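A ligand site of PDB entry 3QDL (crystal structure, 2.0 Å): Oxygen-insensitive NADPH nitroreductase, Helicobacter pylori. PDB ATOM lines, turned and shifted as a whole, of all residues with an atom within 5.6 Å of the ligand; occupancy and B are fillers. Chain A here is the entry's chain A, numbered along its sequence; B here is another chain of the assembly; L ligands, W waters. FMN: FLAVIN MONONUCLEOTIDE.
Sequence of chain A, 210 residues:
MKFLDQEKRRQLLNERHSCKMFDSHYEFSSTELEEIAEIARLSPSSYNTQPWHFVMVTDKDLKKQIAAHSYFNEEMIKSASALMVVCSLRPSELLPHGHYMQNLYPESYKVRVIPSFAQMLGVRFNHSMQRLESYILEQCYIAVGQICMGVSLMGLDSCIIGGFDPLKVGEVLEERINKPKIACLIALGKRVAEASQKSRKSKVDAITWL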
ATOM      1  N   ARG A  16      -7.682  27.883  32.840  1.00  0.00           N
ATOM      2  CA  ARG A  16      -9.110  27.909  32.560  1.00  0.00           C
ATOM      3  C   ARG A  16      -9.370  26.865  31.480  1.00  0.00           C
ATOM      4  O   ARG A  16      -9.145  27.111  30.293  1.00  0.00           O
ATOM      5  CB  ARG A  16      -9.545  29.305  32.077  1.00  0.00           C
ATOM      6  CG  ARG A  16     -11.016  29.670  32.318  1.00  0.00           C
ATOM      7  CD  ARG A  16     -12.012  28.754  31.604  1.00  0.00           C
ATOM      8  NE  ARG A  16     -11.749  28.661  30.165  1.00  0.00           N
ATOM      9  CZ  ARG A  16     -12.047  27.609  29.418  1.00  0.00           C
ATOM     10  NH1 ARG A  16     -11.768  27.625  28.118  1.00  0.00           N
ATOM     11  NH2 ARG A  16     -12.615  26.536  29.951  1.00  0.00           N
ATOM     12  N   HIS A  17      -9.802  25.680  31.912  1.00  0.00           N
ATOM     13  CA  HIS A  17     -10.042  24.561  31.011  1.00  0.00           C
ATOM     14  C   HIS A  17     -11.232  23.732  31.498  1.00  0.00           C
ATOM     15  O   HIS A  17     -11.653  23.856  32.644  1.00  0.00           O
ATOM     16  CB  HIS A  17      -8.790  23.680  30.889  1.00  0.00           C
ATOM     17  CG  HIS A  17      -8.566  22.778  32.062  1.00  0.00           C
ATOM     18  ND1 HIS A  17      -8.030  23.219  33.250  1.00  0.00           N
ATOM     19  CD2 HIS A  17      -8.816  21.449  32.230  1.00  0.00           C
ATOM     20  CE1 HIS A  17      -7.953  22.207  34.104  1.00  0.00           C
ATOM     21  NE2 HIS A  17      -8.428  21.128  33.499  1.00  0.00           N
ATOM     22  N   SER A  18     -11.765  22.885  30.612  1.00  0.00           N
ATOM     23  CA  SER A  18     -12.869  22.004  30.989  1.00  0.00           C
ATOM     24  C   SER A  18     -12.365  20.772  31.741  1.00  0.00           C
ATOM     25  O   SER A  18     -12.000  19.761  31.128  1.00  0.00           O
ATOM     26  CB  SER A  18     -13.693  21.627  29.768  1.00  0.00           C
ATOM     27  OG  SER A  18     -14.294  22.782  29.223  1.00  0.00           O
ATOM     28  N   LYS A  20     -12.325  17.538  33.374  1.00  0.00           N
ATOM     29  CA  LYS A  20     -13.154  16.358  33.098  1.00  0.00           C
ATOM     30  C   LYS A  20     -13.349  15.443  34.306  1.00  0.00           C
ATOM     31  O   LYS A  20     -14.223  14.571  34.280  1.00  0.00           O
ATOM     32  CB  LYS A  20     -12.570  15.560  31.927  1.00  0.00           C
ATOM     33  CG  LYS A  20     -12.131  16.387  30.709  1.00  0.00           C
ATOM     34  CD  LYS A  20     -13.212  16.507  29.642  1.00  0.00           C
ATOM     35  CE  LYS A  20     -14.111  17.729  29.867  1.00  0.00           C
ATOM     36  NZ  LYS A  20     -14.665  18.237  28.587  1.00  0.00           N
ATOM     37  N   PHE A  72     -23.055  11.018  30.070  1.00  0.00           N
ATOM     38  CA  PHE A  72     -21.605  10.809  30.140  1.00  0.00           C
ATOM     39  C   PHE A  72     -20.899  11.750  31.116  1.00  0.00           C
ATOM     40  O   PHE A  72     -19.706  11.594  31.391  1.00  0.00           O
ATOM     41  CB  PHE A  72     -20.968  10.920  28.737  1.00  0.00           C
ATOM     42  CG  PHE A  72     -21.549  12.031  27.893  1.00  0.00           C
ATOM     43  CD1 PHE A  72     -21.003  13.315  27.936  1.00  0.00           C
ATOM     44  CD2 PHE A  72     -22.632  11.796  27.046  1.00  0.00           C
ATOM     45  CE1 PHE A  72     -21.533  14.336  27.152  1.00  0.00           C
ATOM     46  CE2 PHE A  72     -23.175  12.817  26.266  1.00  0.00           C
ATOM     47  CZ  PHE A  72     -22.621  14.090  26.310  1.00  0.00           C
ATOM     48  N   ASN A  73     -21.642  12.731  31.625  1.00  0.00           N
ATOM     49  CA  ASN A  73     -21.121  13.673  32.605  1.00  0.00           C
ATOM     50  C   ASN A  73     -21.345  13.205  34.056  1.00  0.00           C
ATOM     51  O   ASN A  73     -20.924  13.884  34.992  1.00  0.00           O
ATOM     52  CB  ASN A  73     -21.732  15.062  32.390  1.00  0.00           C
ATOM     53  CG  ASN A  73     -21.484  15.602  30.999  1.00  0.00           C
ATOM     54  OD1 ASN A  73     -20.357  15.599  30.500  1.00  0.00           O
ATOM     55  ND2 ASN A  73     -22.546  16.063  30.347  1.00  0.00           N
ATOM     56  N   MET A  76     -18.266  12.688  36.415  1.00  0.00           N
ATOM     57  CA  MET A  76     -17.702  14.030  36.593  1.00  0.00           C
ATOM     58  C   MET A  76     -18.499  14.866  37.610  1.00  0.00           C
ATOM     59  O   MET A  76     -17.920  15.438  38.542  1.00  0.00           O
ATOM     60  CB  MET A  76     -17.593  14.763  35.257  1.00  0.00           C
ATOM     61  CG  MET A  76     -17.349  16.264  35.353  1.00  0.00           C
ATOM     62  SD  MET A  76     -16.941  17.076  33.793  1.00  0.00           S
ATOM     63  CE  MET A  76     -18.414  16.775  32.826  1.00  0.00           C
ATOM     64  N   TYR A 141     -25.034  33.834  30.003  1.00  0.00           N
ATOM     65  CA  TYR A 141     -23.794  33.365  29.386  1.00  0.00           C
ATOM     66  C   TYR A 141     -22.585  34.244  29.710  1.00  0.00           C
ATOM     67  O   TYR A 141     -21.484  33.741  29.906  1.00  0.00           O
ATOM     68  CB  TYR A 141     -23.961  33.225  27.870  1.00  0.00           C
ATOM     69  CG  TYR A 141     -24.512  31.872  27.422  1.00  0.00           C
ATOM     70  CD1 TYR A 141     -24.404  30.730  28.217  1.00  0.00           C
ATOM     71  CD2 TYR A 141     -25.109  31.746  26.169  1.00  0.00           C
ATOM     72  CE1 TYR A 141     -24.900  29.494  27.789  1.00  0.00           C
ATOM     73  CE2 TYR A 141     -25.601  30.513  25.732  1.00  0.00           C
ATOM     74  CZ  TYR A 141     -25.499  29.410  26.536  1.00  0.00           C
ATOM     75  OH  TYR A 141     -25.993  28.208  26.072  1.00  0.00           O
ATOM     76  N   CYS A 159     -16.077  22.990  34.933  1.00  0.00           N
ATOM     77  CA  CYS A 159     -16.497  22.483  33.635  1.00  0.00           C
ATOM     78  C   CYS A 159     -17.948  22.913  33.421  1.00  0.00           C
ATOM     79  O   CYS A 159     -18.830  22.556  34.193  1.00  0.00           O
ATOM     80  CB  CYS A 159     -16.366  20.960  33.551  1.00  0.00           C
ATOM     81  SG  CYS A 159     -16.710  20.264  31.904  1.00  0.00           S
ATOM     82  N   ILE A 160     -18.171  23.714  32.383  1.00  0.00           N
ATOM     83  CA  ILE A 160     -19.521  24.104  31.963  1.00  0.00           C
ATOM     84  C   ILE A 160     -20.183  22.861  31.380  1.00  0.00           C
ATOM     85  O   ILE A 160     -19.564  22.128  30.617  1.00  0.00           O
ATOM     86  CB  ILE A 160     -19.502  25.245  30.905  1.00  0.00           C
ATOM     87  CG1 ILE A 160     -18.660  26.426  31.415  1.00  0.00           C
ATOM     88  CG2 ILE A 160     -20.925  25.694  30.570  1.00  0.00           C
ATOM     89  CD1 ILE A 160     -18.143  27.342  30.317  1.00  0.00           C
ATOM     90  N   ILE A 161     -21.446  22.612  31.747  1.00  0.00           N
ATOM     91  CA  ILE A 161     -22.147  21.396  31.305  1.00  0.00           C
ATOM     92  C   ILE A 161     -23.523  21.686  30.721  1.00  0.00           C
ATOM     93  O   ILE A 161     -24.413  22.214  31.398  1.00  0.00           O
ATOM     94  CB  ILE A 161     -22.240  20.338  32.442  1.00  0.00           C
ATOM     95  CG1 ILE A 161     -20.844  19.840  32.830  1.00  0.00           C
ATOM     96  CG2 ILE A 161     -23.110  19.152  32.011  1.00  0.00           C
ATOM     97  CD1 ILE A 161     -20.756  19.293  34.229  1.00  0.00           C
ATOM     98  N   GLY A 162     -23.689  21.332  29.447  1.00  0.00           N
ATOM     99  CA  GLY A 162     -24.967  21.422  28.747  1.00  0.00           C
ATOM    100  C   GLY A 162     -25.514  20.051  28.379  1.00  0.00           C
ATOM    101  O   GLY A 162     -26.639  19.929  27.913  1.00  0.00           O
ATOM    102  N   GLY A 163     -24.701  19.020  28.594  1.00  0.00           N
ATOM    103  CA  GLY A 163     -25.074  17.646  28.287  1.00  0.00           C
ATOM    104  C   GLY A 163     -25.810  16.977  29.423  1.00  0.00           C
ATOM    105  O   GLY A 163     -25.211  16.220  30.199  1.00  0.00           O
ATOM    106  N   CYS A 184     -27.516  26.475  31.829  1.00  0.00           N
ATOM    107  CA  CYS A 184     -26.434  25.486  31.839  1.00  0.00           C
ATOM    108  C   CYS A 184     -26.024  25.167  33.277  1.00  0.00           C
ATOM    109  O   CYS A 184     -26.437  25.851  34.223  1.00  0.00           O
ATOM    110  CB  CYS A 184     -25.232  25.988  31.042  1.00  0.00           C
ATOM    111  SG  CYS A 184     -24.479  27.484  31.732  1.00  0.00           S
ATOM    112  N   SER A 196      -6.088  19.835  29.971  1.00  0.00           N
ATOM    113  CA  SER A 196      -6.059  19.343  28.597  1.00  0.00           C
ATOM    114  C   SER A 196      -5.486  20.406  27.671  1.00  0.00           C
ATOM    115  O   SER A 196      -5.545  21.590  27.974  1.00  0.00           O
ATOM    116  CB  SER A 196      -7.460  18.941  28.138  1.00  0.00           C
ATOM    117  OG  SER A 196      -8.334  20.069  28.145  1.00  0.00           O
ATOM    118  N   LYS A 198      -5.177  22.972  24.644  1.00  0.00           N
ATOM    119  CA  LYS A 198      -6.108  23.848  23.934  1.00  0.00           C
ATOM    120  C   LYS A 198      -6.229  23.501  22.451  1.00  0.00           C
ATOM    121  O   LYS A 198      -5.219  23.366  21.750  1.00  0.00           O
ATOM    122  CB  LYS A 198      -5.710  25.316  24.119  1.00  0.00           C
ATOM    123  CG  LYS A 198      -6.156  25.936  25.431  1.00  0.00           C
ATOM    124  CD  LYS A 198      -7.592  26.447  25.345  1.00  0.00           C
ATOM    125  CE  LYS A 198      -8.017  27.115  26.636  1.00  0.00           C
ATOM    126  NZ  LYS A 198      -8.452  26.148  27.681  1.00  0.00           N
ATOM    127  N   SER A 199      -7.463  23.355  21.987  1.00  0.00           N
ATOM    128  CA  SER A 199      -7.771  23.134  20.580  1.00  0.00           C
ATOM    129  C   SER A 199      -8.727  24.227  20.103  1.00  0.00           C
ATOM    130  O   SER A 199      -9.906  24.244  20.482  1.00  0.00           O
ATOM    131  CB  SER A 199      -8.388  21.746  20.394  1.00  0.00           C
ATOM    132  OG  SER A 199      -8.607  21.452  19.025  1.00  0.00           O
ATOM    133  N   ARG A 200      -8.214  25.154  19.303  1.00  0.00           N
ATOM    134  CA  ARG A 200      -9.012  26.258  18.762  1.00  0.00           C
ATOM    135  C   ARG A 200      -8.706  26.495  17.285  1.00  0.00           C
ATOM    136  O   ARG A 200      -7.569  26.279  16.844  1.00  0.00           O
ATOM    137  CB  ARG A 200      -8.753  27.561  19.530  1.00  0.00           C
ATOM    138  CG  ARG A 200      -9.110  27.539  21.011  1.00  0.00           C
ATOM    139  CD  ARG A 200     -10.613  27.484  21.245  1.00  0.00           C
ATOM    140  NE  ARG A 200     -10.954  27.778  22.644  1.00  0.00           N
ATOM    141  CZ  ARG A 200     -10.940  26.887  23.620  1.00  0.00           C
ATOM    142  NH1 ARG A 200     -10.587  25.620  23.396  1.00  0.00           N
ATOM    143  NH2 ARG A 200     -11.265  27.257  24.861  1.00  0.00           N
ATOM    144  N   LEU B  42      -9.496  31.846  22.955  1.00  0.00           N
ATOM    145  CA  LEU B  42      -9.388  30.713  23.872  1.00  0.00           C
ATOM    146  C   LEU B  42     -10.617  30.520  24.763  1.00  0.00           C
ATOM    147  O   LEU B  42     -10.595  29.736  25.706  1.00  0.00           O
ATOM    148  CB  LEU B  42      -8.114  30.814  24.724  1.00  0.00           C
ATOM    149  CG  LEU B  42      -6.734  30.888  24.047  1.00  0.00           C
ATOM    150  CD1 LEU B  42      -5.633  30.665  25.069  1.00  0.00           C
ATOM    151  CD2 LEU B  42      -6.584  29.917  22.887  1.00  0.00           C
ATOM    152  N   SER B  43     -11.705  31.241  24.463  1.00  0.00           N
ATOM    153  CA  SER B  43     -12.955  31.106  25.194  1.00  0.00           C
ATOM    154  C   SER B  43     -13.632  29.751  24.960  1.00  0.00           C
ATOM    155  O   SER B  43     -13.416  29.129  23.911  1.00  0.00           O
ATOM    156  CB  SER B  43     -13.917  32.238  24.820  1.00  0.00           C
ATOM    157  OG  SER B  43     -13.516  33.463  25.417  1.00  0.00           O
ATOM    158  N   PRO B  44     -14.433  29.284  25.933  1.00  0.00           N
ATOM    159  CA  PRO B  44     -15.093  27.976  25.830  1.00  0.00           C
ATOM    160  C   PRO B  44     -16.478  28.019  25.163  1.00  0.00           C
ATOM    161  O   PRO B  44     -17.163  29.040  25.219  1.00  0.00           O
ATOM    162  CB  PRO B  44     -15.212  27.539  27.291  1.00  0.00           C
ATOM    163  CG  PRO B  44     -15.289  28.800  28.071  1.00  0.00           C
ATOM    164  CD  PRO B  44     -14.659  29.903  27.260  1.00  0.00           C
ATOM    165  N   SER B  45     -16.871  26.902  24.557  1.00  0.00           N
ATOM    166  CA  SER B  45     -18.155  26.789  23.861  1.00  0.00           C
ATOM    167  C   SER B  45     -18.558  25.322  23.733  1.00  0.00           C
ATOM    168  O   SER B  45     -17.717  24.425  23.864  1.00  0.00           O
ATOM    169  CB  SER B  45     -18.080  27.426  22.475  1.00  0.00           C
ATOM    170  OG  SER B  45     -17.127  26.767  21.673  1.00  0.00           O
ATOM    171  N   SER B  46     -19.854  25.087  23.469  1.00  0.00           N
ATOM    172  CA  SER B  46     -20.409  23.738  23.341  1.00  0.00           C
ATOM    173  C   SER B  46     -19.615  22.925  22.318  1.00  0.00           C
ATOM    174  O   SER B  46     -19.449  23.360  21.181  1.00  0.00           O
ATOM    175  CB  SER B  46     -21.876  23.778  22.912  1.00  0.00           C
ATOM    176  OG  SER B  46     -22.670  24.521  23.829  1.00  0.00           O
ATOM    177  N   TYR B  47     -19.131  21.767  22.749  1.00  0.00           N
ATOM    178  CA  TYR B  47     -18.379  20.835  21.891  1.00  0.00           C
ATOM    179  C   TYR B  47     -17.183  21.486  21.185  1.00  0.00           C
ATOM    180  O   TYR B  47     -16.693  20.980  20.171  1.00  0.00           O
ATOM    181  CB  TYR B  47     -19.304  20.177  20.857  1.00  0.00           C
ATOM    182  CG  TYR B  47     -20.484  19.441  21.439  1.00  0.00           C
ATOM    183  CD1 TYR B  47     -20.367  18.112  21.860  1.00  0.00           C
ATOM    184  CD2 TYR B  47     -21.733  20.055  21.561  1.00  0.00           C
ATOM    185  CE1 TYR B  47     -21.453  17.420  22.389  1.00  0.00           C
ATOM    186  CE2 TYR B  47     -22.828  19.374  22.090  1.00  0.00           C
ATOM    187  CZ  TYR B  47     -22.678  18.058  22.497  1.00  0.00           C
ATOM    188  OH  TYR B  47     -23.758  17.388  23.025  1.00  0.00           O
ATOM    189  N   ASN B  48     -16.727  22.608  21.733  1.00  0.00           N
ATOM    190  CA  ASN B  48     -15.650  23.419  21.141  1.00  0.00           C
ATOM    191  C   ASN B  48     -16.008  23.897  19.724  1.00  0.00           C
ATOM    192  O   ASN B  48     -15.148  23.954  18.844  1.00  0.00           O
ATOM    193  CB  ASN B  48     -14.327  22.642  21.162  1.00  0.00           C
ATOM    194  CG  ASN B  48     -13.115  23.531  20.920  1.00  0.00           C
ATOM    195  OD1 ASN B  48     -13.019  24.643  21.454  1.00  0.00           O
ATOM    196  ND2 ASN B  48     -12.182  23.032  20.122  1.00  0.00           N
ATOM    197  N   GLN B 139     -23.462  31.895  22.266  1.00  0.00           N
ATOM    198  CA  GLN B 139     -22.300  31.580  23.115  1.00  0.00           C
ATOM    199  C   GLN B 139     -21.096  32.484  22.920  1.00  0.00           C
ATOM    200  O   GLN B 139     -20.083  32.321  23.614  1.00  0.00           O
ATOM    201  CB  GLN B 139     -21.918  30.107  22.985  1.00  0.00           C
ATOM    202  CG  GLN B 139     -22.982  29.175  23.558  1.00  0.00           C
ATOM    203  CD  GLN B 139     -22.627  27.713  23.464  1.00  0.00           C
ATOM    204  OE1 GLN B 139     -21.505  27.352  23.076  1.00  0.00           O
ATOM    205  NE2 GLN B 139     -23.578  26.851  23.814  1.00  0.00           N
ATOM    206  N   ILE B 142     -20.449  34.096  26.177  1.00  0.00           N
ATOM    207  CA  ILE B 142     -19.529  33.438  27.116  1.00  0.00           C
ATOM    208  C   ILE B 142     -18.121  34.020  26.946  1.00  0.00           C
ATOM    209  O   ILE B 142     -17.404  34.225  27.923  1.00  0.00           O
ATOM    210  CB  ILE B 142     -19.503  31.897  26.956  1.00  0.00           C
ATOM    211  CG1 ILE B 142     -20.807  31.287  27.508  1.00  0.00           C
ATOM    212  CG2 ILE B 142     -18.306  31.278  27.694  1.00  0.00           C
ATOM    213  CD1 ILE B 142     -21.041  29.845  27.066  1.00  0.00           C
HETATM  214  N1  FMN L   1     -17.766  19.614  28.482  1.00  0.00           N
HETATM  215  C2  FMN L   1     -18.095  18.324  28.856  1.00  0.00           C
HETATM  216  O2  FMN L   1     -17.203  17.503  29.062  1.00  0.00           O
HETATM  217  N3  FMN L   1     -19.415  17.948  28.996  1.00  0.00           N
HETATM  218  C4  FMN L   1     -20.421  18.870  28.770  1.00  0.00           C
HETATM  219  O4  FMN L   1     -21.600  18.531  28.894  1.00  0.00           O
HETATM  220  C4A FMN L   1     -20.096  20.174  28.387  1.00  0.00           C
HETATM  221  N5  FMN L   1     -21.097  21.089  28.149  1.00  0.00           N
HETATM  222  C5A FMN L   1     -20.796  22.378  27.783  1.00  0.00           C
HETATM  223  C6  FMN L   1     -21.844  23.280  27.563  1.00  0.00           C
HETATM  224  C7  FMN L   1     -21.567  24.594  27.191  1.00  0.00           C
HETATM  225  C7M FMN L   1     -22.715  25.528  26.960  1.00  0.00           C
HETATM  226  C8  FMN L   1     -20.244  25.006  27.040  1.00  0.00           C
HETATM  227  C8M FMN L   1     -19.911  26.409  26.644  1.00  0.00           C
HETATM  228  C9  FMN L   1     -19.201  24.101  27.269  1.00  0.00           C
HETATM  229  C9A FMN L   1     -19.464  22.778  27.633  1.00  0.00           C
HETATM  230  N10 FMN L   1     -18.437  21.854  27.859  1.00  0.00           N
HETATM  231  C10 FMN L   1     -18.762  20.550  28.242  1.00  0.00           C
HETATM  232  C1' FMN L   1     -16.981  22.230  27.723  1.00  0.00           C
HETATM  233  C2' FMN L   1     -16.527  22.417  26.265  1.00  0.00           C
HETATM  234  O2' FMN L   1     -16.513  21.164  25.595  1.00  0.00           O
HETATM  235  C3' FMN L   1     -15.133  23.060  26.226  1.00  0.00           C
HETATM  236  O3' FMN L   1     -15.212  24.389  26.694  1.00  0.00           O
HETATM  237  C4' FMN L   1     -14.455  23.073  24.851  1.00  0.00           C
HETATM  238  O4' FMN L   1     -14.232  21.743  24.416  1.00  0.00           O
HETATM  239  C5' FMN L   1     -13.128  23.821  24.890  1.00  0.00           C
HETATM  240  O5' FMN L   1     -12.234  23.231  25.823  1.00  0.00           O
HETATM  241  P   FMN L   1     -11.661  24.042  27.100  1.00  0.00           P
HETATM  242  O1P FMN L   1     -11.004  23.051  28.013  1.00  0.00           O
HETATM  243  O2P FMN L   1     -12.777  24.737  27.834  1.00  0.00           O
HETATM  244  O3P FMN L   1     -10.652  25.075  26.647  1.00  0.00           O
HETATM  245  O   HOH W   1      -9.471  23.044  24.151  1.00  0.00           O
HETATM  246  O   HOH W   2     -16.351  24.021  30.302  1.00  0.00           O
HETATM  247  O   HOH W   3      -8.557  22.849  26.658  1.00  0.00           O
HETATM  248  O   HOH W   4     -19.094  19.523  25.012  1.00  0.00           O
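The side-chain amino group of Lys 198 lies within salt-bridge range of an oxygen (O3P) of the ligand (2.7 Å). NZ of Lys 20 sits at hydrogen-bond distance from O2 of the ligand, at 2.7 Å. An oxygen (O1P) of the ligand is in hydrogen-bond range of the backbone NH (N) of Ser 18, at 2.7 Å. OG of Ser 18 is in hydrogen-bond range of O2P of the ligand, at 2.8 Å. O2P of the ligand is in salt-bridge range of NH2 of Arg 16, 2.8 Å away. The guanidinium group (NH2) of Arg 200 is in salt-bridge range of an oxygen (O3P) of the ligand. N of Gly 162 lies within hydrogen-bond range of N5 of the ligand. A nitrogen (N3) of the ligand is in hydrogen-bond range of the side-chain amide oxygen of Asn 73 (2.9 Å). N of Gly 163 lies within hydrogen-bond range of O4 of the ligand (3.2 Å). The side-chain sulfur (SG) of Cys 159 sits at hydrogen-bond distance from a nitrogen (N1) of the ligand (3.6 Å).
The side-chain amino group of Lys 198 is in hydrogen-bond range of the backbone carbonyl oxygen of Arg 16 (2.9 Å). The backbone carbonyl oxygen (O) of Leu 42 of chain B is in hydrogen-bond range of the guanidinium group (NH1) of Arg 16. NH1 of Arg 200 is in hydrogen-bond range of OD1 of Asn 48 of chain B (3.3 Å). O of Leu 42 of chain B is in hydrogen-bond range of NH2 of Arg 200, 2.7 Å away. The backbone carbonyl oxygen of Ser 43 of chain B sits at hydrogen-bond distance from the guanidinium group of Arg 200 (3.0 Å). The side-chain amide nitrogen of Asn 73 lies within hydrogen-bond range of the backbone carbonyl oxygen of Gly 163, 2.7 Å away. NE2 of Gln 139 of chain B lies within hydrogen-bond range of OG of Ser 46 of chain B (2.5 Å). The backbone carbonyl oxygen of Ser 199 is in hydrogen-bond range of the side-chain amide nitrogen of Asn 48 of chain B (2.6 Å).
A nitrogen (N10) of the ligand lies close to the backbone carbonyl oxygen of Ile 160 (3.0 Å). Residues that only touch the ligand: Pro 44 of chain B (3.2 Å), Ser 46 of chain B (3.3 Å), Ser 45 of chain B (3.3 Å), Ile 161 (3.3 Å), Asn 48 of chain B (3.4 Å), His 17 (3.5 Å), Gln 139 of chain B (3.5 Å), Ile 142 of chain B (3.6 Å) and Tyr 47 of chain B (3.9 Å). Hydrophobic or aromatic side chains that line the ligand: His 17, Ile 160, Ile 161, Pro 44 of chain B and Ile 142 of chain B.
Water W3 lies within hydrogen-bond range of O1P of the ligand, OG of Ser 196 and NZ of Lys 198. Water W4 lies within hydrogen-bond range of an oxygen (O2') of the ligand (3.1 Å) and the backbone NH of Tyr 47 of chain B (3.2 Å). Water W2 lies within hydrogen-bond range of OG of Ser 18 (2.6 Å) and N of Ile 160 (2.8 Å). Water W1 lies within hydrogen-bond range of NH1 of Arg 200 (2.9 Å), N of Ser 199 (3.0 Å) and O5' of the ligand (3.2 Å).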
